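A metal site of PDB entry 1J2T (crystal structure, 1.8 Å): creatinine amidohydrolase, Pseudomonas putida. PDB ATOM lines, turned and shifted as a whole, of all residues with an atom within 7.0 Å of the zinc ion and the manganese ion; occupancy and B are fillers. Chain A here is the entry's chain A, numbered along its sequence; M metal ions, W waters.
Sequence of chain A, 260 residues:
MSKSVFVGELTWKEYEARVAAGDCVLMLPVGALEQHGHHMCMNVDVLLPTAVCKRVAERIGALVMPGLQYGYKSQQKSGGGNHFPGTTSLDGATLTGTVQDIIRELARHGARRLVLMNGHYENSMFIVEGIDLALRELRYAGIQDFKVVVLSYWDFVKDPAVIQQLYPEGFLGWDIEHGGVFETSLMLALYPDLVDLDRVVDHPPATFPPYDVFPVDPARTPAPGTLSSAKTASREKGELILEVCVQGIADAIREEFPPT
Within 4 Å of the manganese ion: Glu 34, Asp 45 and His 120. The nearest printed residue that does not touch the manganese ion is His 178 (4.1 Å).
NE2 of His 178 is in hydrogen-bond range of O of Gln 35 (2.9 Å). NE2 of His 178 sits at hydrogen-bond distance from O of Gly 79 (3.3 Å). NE2 of His 120 is in hydrogen-bond range of O of Tyr 72, 2.8 Å away. A ring nitrogen (ND1) of His 36 is in hydrogen-bond range of the backbone carbonyl oxygen (O) of Glu 34. The side-chain carboxylate (OE2) of Glu 183 lies within hydrogen-bond range of the backbone NH (N) of Gly 179, 2.9 Å away. The side-chain carboxylate of Glu 34 sits at hydrogen-bond distance from the side-chain hydroxyl of Ser 74, 3.2 Å away. A ring nitrogen (NE2) of His 120 lies close to the side-chain carboxylate (OE1) of Glu 122 (3.3 Å).
The manganese ion is bound by OD2 of Asp 45 (2.0 Å), OE2 of Glu 34 (2.1 Å), water W1 (2.2 Å), water W3 (2.2 Å) and ND1 of His 120 (2.3 Å).
The zinc ion is bound by water W3, the side-chain carboxylate (OD1) of Asp 45, the side-chain carboxylate (OE1) of Glu 183 and a ring nitrogen (NE2) of His 36. The zinc ion has four donor atoms within binding distance. Slightly farther from the zinc ion lies OE2 of Glu 183 (2.8 Å).
Merely in contact with the zinc ion: His 178 (3.9 Å). Within 4 Å of the zinc ion: His 36, Asp 45, His 178 and Glu 183.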
ATOM      1  N   GLY A  31     -33.918 -14.694 -10.917  1.00  0.00           N
ATOM      2  CA  GLY A  31     -32.510 -15.000 -10.910  1.00  0.00           C
ATOM      3  C   GLY A  31     -31.534 -13.880 -11.228  1.00  0.00           C
ATOM      4  O   GLY A  31     -31.676 -12.755 -10.752  1.00  0.00           O
ATOM      5  N   ALA A  32     -30.511 -14.227 -12.014  1.00  0.00           N
ATOM      6  CA  ALA A  32     -29.420 -13.320 -12.354  1.00  0.00           C
ATOM      7  C   ALA A  32     -28.519 -13.962 -13.416  1.00  0.00           C
ATOM      8  O   ALA A  32     -28.535 -15.172 -13.610  1.00  0.00           O
ATOM      9  CB  ALA A  32     -28.569 -12.986 -11.114  1.00  0.00           C
ATOM     10  N   GLU A  34     -24.668 -14.051 -13.811  1.00  0.00           N
ATOM     11  CA  GLU A  34     -23.605 -13.707 -12.897  1.00  0.00           C
ATOM     12  C   GLU A  34     -22.486 -14.734 -12.916  1.00  0.00           C
ATOM     13  O   GLU A  34     -22.717 -15.925 -13.021  1.00  0.00           O
ATOM     14  CB  GLU A  34     -24.191 -13.614 -11.469  1.00  0.00           C
ATOM     15  CG  GLU A  34     -23.192 -13.301 -10.356  1.00  0.00           C
ATOM     16  CD  GLU A  34     -23.831 -13.452  -8.982  1.00  0.00           C
ATOM     17  OE1 GLU A  34     -23.626 -12.578  -8.136  1.00  0.00           O
ATOM     18  OE2 GLU A  34     -24.547 -14.445  -8.765  1.00  0.00           O
ATOM     19  N   GLN A  35     -21.255 -14.250 -12.831  1.00  0.00           N
ATOM     20  CA  GLN A  35     -20.110 -15.137 -12.765  1.00  0.00           C
ATOM     21  C   GLN A  35     -20.281 -16.119 -11.606  1.00  0.00           C
ATOM     22  O   GLN A  35     -20.738 -15.755 -10.503  1.00  0.00           O
ATOM     23  CB  GLN A  35     -18.818 -14.318 -12.569  1.00  0.00           C
ATOM     24  CG  GLN A  35     -18.670 -13.610 -11.182  1.00  0.00           C
ATOM     25  CD  GLN A  35     -18.151 -14.529 -10.066  1.00  0.00           C
ATOM     26  OE1 GLN A  35     -17.549 -15.565 -10.332  1.00  0.00           O
ATOM     27  NE2 GLN A  35     -18.358 -14.114  -8.801  1.00  0.00           N
ATOM     28  N   HIS A  36     -19.882 -17.367 -11.850  1.00  0.00           N
ATOM     29  CA  HIS A  36     -19.903 -18.412 -10.834  1.00  0.00           C
ATOM     30  C   HIS A  36     -18.606 -19.239 -10.884  1.00  0.00           C
ATOM     31  O   HIS A  36     -18.622 -20.479 -10.973  1.00  0.00           O
ATOM     32  CB  HIS A  36     -21.117 -19.314 -11.038  1.00  0.00           C
ATOM     33  CG  HIS A  36     -22.368 -18.782 -10.425  1.00  0.00           C
ATOM     34  ND1 HIS A  36     -23.124 -17.780 -11.006  1.00  0.00           N
ATOM     35  CD2 HIS A  36     -23.009 -19.119  -9.279  1.00  0.00           C
ATOM     36  CE1 HIS A  36     -24.164 -17.523 -10.241  1.00  0.00           C
ATOM     37  NE2 HIS A  36     -24.123 -18.329  -9.191  1.00  0.00           N
ATOM     38  N   MET A  40     -18.213 -23.278 -13.437  1.00  0.00           N
ATOM     39  CA  MET A  40     -19.644 -23.314 -13.647  1.00  0.00           C
ATOM     40  C   MET A  40     -20.081 -22.141 -14.513  1.00  0.00           C
ATOM     41  O   MET A  40     -19.429 -21.112 -14.522  1.00  0.00           O
ATOM     42  CB  MET A  40     -20.344 -23.178 -12.291  1.00  0.00           C
ATOM     43  CG  MET A  40     -21.644 -23.854 -12.185  1.00  0.00           C
ATOM     44  SD  MET A  40     -22.032 -24.256 -10.513  1.00  0.00           S
ATOM     45  CE  MET A  40     -21.329 -22.809  -9.582  1.00  0.00           C
ATOM     46  N   VAL A  44     -26.725 -19.895 -13.530  1.00  0.00           N
ATOM     47  CA  VAL A  44     -27.064 -20.718 -12.364  1.00  0.00           C
ATOM     48  C   VAL A  44     -28.265 -20.203 -11.569  1.00  0.00           C
ATOM     49  O   VAL A  44     -29.179 -20.968 -11.236  1.00  0.00           O
ATOM     50  CB  VAL A  44     -25.819 -20.873 -11.443  1.00  0.00           C
ATOM     51  CG1 VAL A  44     -26.219 -21.425 -10.043  1.00  0.00           C
ATOM     52  CG2 VAL A  44     -24.775 -21.769 -12.104  1.00  0.00           C
ATOM     53  N   ASP A  45     -28.284 -18.899 -11.302  1.00  0.00           N
ATOM     54  CA  ASP A  45     -29.324 -18.321 -10.436  1.00  0.00           C
ATOM     55  C   ASP A  45     -30.712 -18.319 -11.069  1.00  0.00           C
ATOM     56  O   ASP A  45     -31.697 -18.080 -10.370  1.00  0.00           O
ATOM     57  CB  ASP A  45     -28.961 -16.900  -9.971  1.00  0.00           C
ATOM     58  CG  ASP A  45     -27.760 -16.866  -9.020  1.00  0.00           C
ATOM     59  OD1 ASP A  45     -27.191 -17.948  -8.671  1.00  0.00           O
ATOM     60  OD2 ASP A  45     -27.332 -15.786  -8.545  1.00  0.00           O
ATOM     61  N   LEU A  48     -31.477 -22.818 -11.276  1.00  0.00           N
ATOM     62  CA  LEU A  48     -31.761 -23.532 -10.034  1.00  0.00           C
ATOM     63  C   LEU A  48     -33.166 -23.274  -9.470  1.00  0.00           C
ATOM     64  O   LEU A  48     -33.926 -24.238  -9.284  1.00  0.00           O
ATOM     65  CB  LEU A  48     -30.649 -23.266  -9.005  1.00  0.00           C
ATOM     66  CG  LEU A  48     -29.296 -23.858  -9.455  1.00  0.00           C
ATOM     67  CD1 LEU A  48     -28.233 -23.724  -8.376  1.00  0.00           C
ATOM     68  CD2 LEU A  48     -29.394 -25.324  -9.925  1.00  0.00           C
ATOM     69  N   TYR A  72     -30.297  -7.969  -9.442  1.00  0.00           N
ATOM     70  CA  TYR A  72     -29.588  -6.842  -8.861  1.00  0.00           C
ATOM     71  C   TYR A  72     -28.071  -7.058  -8.870  1.00  0.00           C
ATOM     72  O   TYR A  72     -27.579  -8.201  -8.934  1.00  0.00           O
ATOM     73  CB  TYR A  72     -30.100  -6.513  -7.448  1.00  0.00           C
ATOM     74  CG  TYR A  72     -29.482  -5.219  -6.946  1.00  0.00           C
ATOM     75  CD1 TYR A  72     -29.748  -4.019  -7.591  1.00  0.00           C
ATOM     76  CD2 TYR A  72     -28.569  -5.219  -5.901  1.00  0.00           C
ATOM     77  CE1 TYR A  72     -29.149  -2.832  -7.161  1.00  0.00           C
ATOM     78  CE2 TYR A  72     -27.979  -4.058  -5.477  1.00  0.00           C
ATOM     79  CZ  TYR A  72     -28.265  -2.868  -6.116  1.00  0.00           C
ATOM     80  OH  TYR A  72     -27.650  -1.721  -5.703  1.00  0.00           O
ATOM     81  N   SER A  74     -24.385  -7.694  -8.237  1.00  0.00           N
ATOM     82  CA  SER A  74     -23.612  -8.569  -7.389  1.00  0.00           C
ATOM     83  C   SER A  74     -22.853  -7.758  -6.332  1.00  0.00           C
ATOM     84  O   SER A  74     -22.257  -6.720  -6.651  1.00  0.00           O
ATOM     85  CB  SER A  74     -22.634  -9.377  -8.256  1.00  0.00           C
ATOM     86  OG  SER A  74     -21.739 -10.121  -7.457  1.00  0.00           O
ATOM     87  N   SER A  78     -21.382 -11.276  -1.083  1.00  0.00           N
ATOM     88  CA  SER A  78     -22.382 -12.296  -1.412  1.00  0.00           C
ATOM     89  C   SER A  78     -22.390 -12.857  -2.845  1.00  0.00           C
ATOM     90  O   SER A  78     -23.105 -13.817  -3.131  1.00  0.00           O
ATOM     91  CB  SER A  78     -23.785 -11.775  -1.083  1.00  0.00           C
ATOM     92  OG  SER A  78     -23.988 -10.501  -1.673  1.00  0.00           O
ATOM     93  N   GLY A  79     -21.609 -12.266  -3.757  1.00  0.00           N
ATOM     94  CA  GLY A  79     -21.566 -12.733  -5.141  1.00  0.00           C
ATOM     95  C   GLY A  79     -20.280 -12.432  -5.911  1.00  0.00           C
ATOM     96  O   GLY A  79     -20.224 -12.574  -7.131  1.00  0.00           O
ATOM     97  N   GLY A 119     -33.373 -16.749  -6.527  1.00  0.00           N
ATOM     98  CA  GLY A 119     -32.176 -17.561  -6.674  1.00  0.00           C
ATOM     99  C   GLY A 119     -30.873 -16.794  -6.603  1.00  0.00           C
ATOM    100  O   GLY A 119     -29.808 -17.404  -6.681  1.00  0.00           O
ATOM    101  N   HIS A 120     -30.942 -15.468  -6.470  1.00  0.00           N
ATOM    102  CA  HIS A 120     -29.768 -14.585  -6.430  1.00  0.00           C
ATOM    103  C   HIS A 120     -29.862 -13.750  -5.169  1.00  0.00           C
ATOM    104  O   HIS A 120     -30.785 -12.961  -5.004  1.00  0.00           O
ATOM    105  CB  HIS A 120     -29.744 -13.726  -7.685  1.00  0.00           C
ATOM    106  CG  HIS A 120     -28.676 -12.673  -7.716  1.00  0.00           C
ATOM    107  ND1 HIS A 120     -27.328 -12.971  -7.727  1.00  0.00           N
ATOM    108  CD2 HIS A 120     -28.766 -11.330  -7.839  1.00  0.00           C
ATOM    109  CE1 HIS A 120     -26.632 -11.853  -7.831  1.00  0.00           C
ATOM    110  NE2 HIS A 120     -27.481 -10.838  -7.910  1.00  0.00           N
ATOM    111  N   TYR A 121     -28.889 -13.955  -4.283  1.00  0.00           N
ATOM    112  CA  TYR A 121     -28.921 -13.411  -2.922  1.00  0.00           C
ATOM    113  C   TYR A 121     -29.294 -11.936  -2.853  1.00  0.00           C
ATOM    114  O   TYR A 121     -30.147 -11.541  -2.049  1.00  0.00           O
ATOM    115  CB  TYR A 121     -27.552 -13.611  -2.258  1.00  0.00           C
ATOM    116  CG  TYR A 121     -27.556 -13.399  -0.769  1.00  0.00           C
ATOM    117  CD1 TYR A 121     -27.753 -14.470   0.103  1.00  0.00           C
ATOM    118  CD2 TYR A 121     -27.381 -12.133  -0.221  1.00  0.00           C
ATOM    119  CE1 TYR A 121     -27.750 -14.293   1.464  1.00  0.00           C
ATOM    120  CE2 TYR A 121     -27.394 -11.946   1.155  1.00  0.00           C
ATOM    121  CZ  TYR A 121     -27.580 -13.036   1.993  1.00  0.00           C
ATOM    122  OH  TYR A 121     -27.590 -12.897   3.370  1.00  0.00           O
ATOM    123  N   GLU A 122     -28.705 -11.144  -3.746  1.00  0.00           N
ATOM    124  CA  GLU A 122     -28.864  -9.692  -3.749  1.00  0.00           C
ATOM    125  C   GLU A 122     -30.237  -9.181  -4.162  1.00  0.00           C
ATOM    126  O   GLU A 122     -30.542  -8.019  -3.933  1.00  0.00           O
ATOM    127  CB  GLU A 122     -27.811  -9.082  -4.692  1.00  0.00           C
ATOM    128  CG  GLU A 122     -26.390  -9.141  -4.165  1.00  0.00           C
ATOM    129  CD  GLU A 122     -25.695 -10.450  -4.460  1.00  0.00           C
ATOM    130  OE1 GLU A 122     -26.378 -11.429  -4.817  1.00  0.00           O
ATOM    131  OE2 GLU A 122     -24.458 -10.513  -4.307  1.00  0.00           O
ATOM    132  N   TYR A 153     -34.742 -20.089  -2.094  1.00  0.00           N
ATOM    133  CA  TYR A 153     -34.886 -21.547  -1.970  1.00  0.00           C
ATOM    134  C   TYR A 153     -33.909 -22.199  -0.982  1.00  0.00           C
ATOM    135  O   TYR A 153     -34.276 -23.174  -0.302  1.00  0.00           O
ATOM    136  CB  TYR A 153     -34.887 -22.260  -3.339  1.00  0.00           C
ATOM    137  CG  TYR A 153     -33.549 -22.273  -4.031  1.00  0.00           C
ATOM    138  CD1 TYR A 153     -32.668 -23.331  -3.870  1.00  0.00           C
ATOM    139  CD2 TYR A 153     -33.147 -21.206  -4.835  1.00  0.00           C
ATOM    140  CE1 TYR A 153     -31.448 -23.356  -4.468  1.00  0.00           C
ATOM    141  CE2 TYR A 153     -31.889 -21.211  -5.443  1.00  0.00           C
ATOM    142  CZ  TYR A 153     -31.045 -22.293  -5.255  1.00  0.00           C
ATOM    143  OH  TYR A 153     -29.811 -22.319  -5.836  1.00  0.00           O
ATOM    144  N   TRP A 154     -32.697 -21.663  -0.865  1.00  0.00           N
ATOM    145  CA  TRP A 154     -31.709 -22.242   0.050  1.00  0.00           C
ATOM    146  C   TRP A 154     -32.107 -22.143   1.521  1.00  0.00           C
ATOM    147  O   TRP A 154     -31.675 -22.960   2.322  1.00  0.00           O
ATOM    148  CB  TRP A 154     -30.331 -21.623  -0.151  1.00  0.00           C
ATOM    149  CG  TRP A 154     -30.329 -20.138  -0.087  1.00  0.00           C
ATOM    150  CD1 TRP A 154     -30.347 -19.354   1.021  1.00  0.00           C
ATOM    151  CD2 TRP A 154     -30.358 -19.259  -1.209  1.00  0.00           C
ATOM    152  NE1 TRP A 154     -30.349 -18.027   0.662  1.00  0.00           N
ATOM    153  CE2 TRP A 154     -30.355 -17.943  -0.709  1.00  0.00           C
ATOM    154  CE3 TRP A 154     -30.343 -19.452  -2.593  1.00  0.00           C
ATOM    155  CZ2 TRP A 154     -30.363 -16.832  -1.534  1.00  0.00           C
ATOM    156  CZ3 TRP A 154     -30.357 -18.347  -3.413  1.00  0.00           C
ATOM    157  CH2 TRP A 154     -30.364 -17.049  -2.887  1.00  0.00           C
ATOM    158  N   GLU A 177     -21.897 -18.370   0.548  1.00  0.00           N
ATOM    159  CA  GLU A 177     -22.156 -19.417  -0.400  1.00  0.00           C
ATOM    160  C   GLU A 177     -22.405 -18.761  -1.745  1.00  0.00           C
ATOM    161  O   GLU A 177     -23.517 -18.307  -2.034  1.00  0.00           O
ATOM    162  CB  GLU A 177     -23.408 -20.229  -0.051  1.00  0.00           C
ATOM    163  CG  GLU A 177     -23.162 -21.555   0.643  1.00  0.00           C
ATOM    164  CD  GLU A 177     -22.080 -22.391   0.005  1.00  0.00           C
ATOM    165  OE1 GLU A 177     -21.003 -22.467   0.629  1.00  0.00           O
ATOM    166  OE2 GLU A 177     -22.302 -22.986  -1.095  1.00  0.00           O
ATOM    167  N   HIS A 178     -21.355 -18.661  -2.534  1.00  0.00           N
ATOM    168  CA  HIS A 178     -21.513 -18.239  -3.916  1.00  0.00           C
ATOM    169  C   HIS A 178     -20.572 -19.104  -4.741  1.00  0.00           C
ATOM    170  O   HIS A 178     -19.369 -19.026  -4.595  1.00  0.00           O
ATOM    171  CB  HIS A 178     -21.202 -16.756  -4.123  1.00  0.00           C
ATOM    172  CG  HIS A 178     -21.215 -16.366  -5.569  1.00  0.00           C
ATOM    173  ND1 HIS A 178     -22.352 -16.415  -6.337  1.00  0.00           N
ATOM    174  CD2 HIS A 178     -20.221 -15.967  -6.397  1.00  0.00           C
ATOM    175  CE1 HIS A 178     -22.057 -16.061  -7.575  1.00  0.00           C
ATOM    176  NE2 HIS A 178     -20.772 -15.783  -7.637  1.00  0.00           N
ATOM    177  N   GLY A 179     -21.162 -19.945  -5.596  1.00  0.00           N
ATOM    178  CA  GLY A 179     -20.413 -20.830  -6.466  1.00  0.00           C
ATOM    179  C   GLY A 179     -19.710 -21.934  -5.715  1.00  0.00           C
ATOM    180  O   GLY A 179     -18.790 -22.570  -6.236  1.00  0.00           O
ATOM    181  N   GLU A 183     -24.518 -24.615  -4.619  1.00  0.00           N
ATOM    182  CA  GLU A 183     -24.924 -24.437  -6.012  1.00  0.00           C
ATOM    183  C   GLU A 183     -24.271 -25.439  -6.934  1.00  0.00           C
ATOM    184  O   GLU A 183     -24.911 -25.947  -7.855  1.00  0.00           O
ATOM    185  CB  GLU A 183     -24.599 -23.021  -6.491  1.00  0.00           C
ATOM    186  CG  GLU A 183     -25.430 -21.954  -5.815  1.00  0.00           C
ATOM    187  CD  GLU A 183     -25.123 -20.560  -6.345  1.00  0.00           C
ATOM    188  OE1 GLU A 183     -26.075 -19.894  -6.797  1.00  0.00           O
ATOM    189  OE2 GLU A 183     -23.938 -20.160  -6.330  1.00  0.00           O
HETATM  190 ZN    ZN M   1     -25.511 -18.219  -7.676  1.00  0.00          ZN
HETATM  191 MN    MN M   2     -26.017 -14.771  -7.359  1.00  0.00          MN
HETATM  192  O   HOH W   1     -25.433 -13.914  -5.472  1.00  0.00           O
HETATM  193  O   HOH W   2     -27.306 -16.373  -4.928  1.00  0.00           O
HETATM  194  O   HOH W   3     -25.256 -16.683  -6.600  1.00  0.00           O
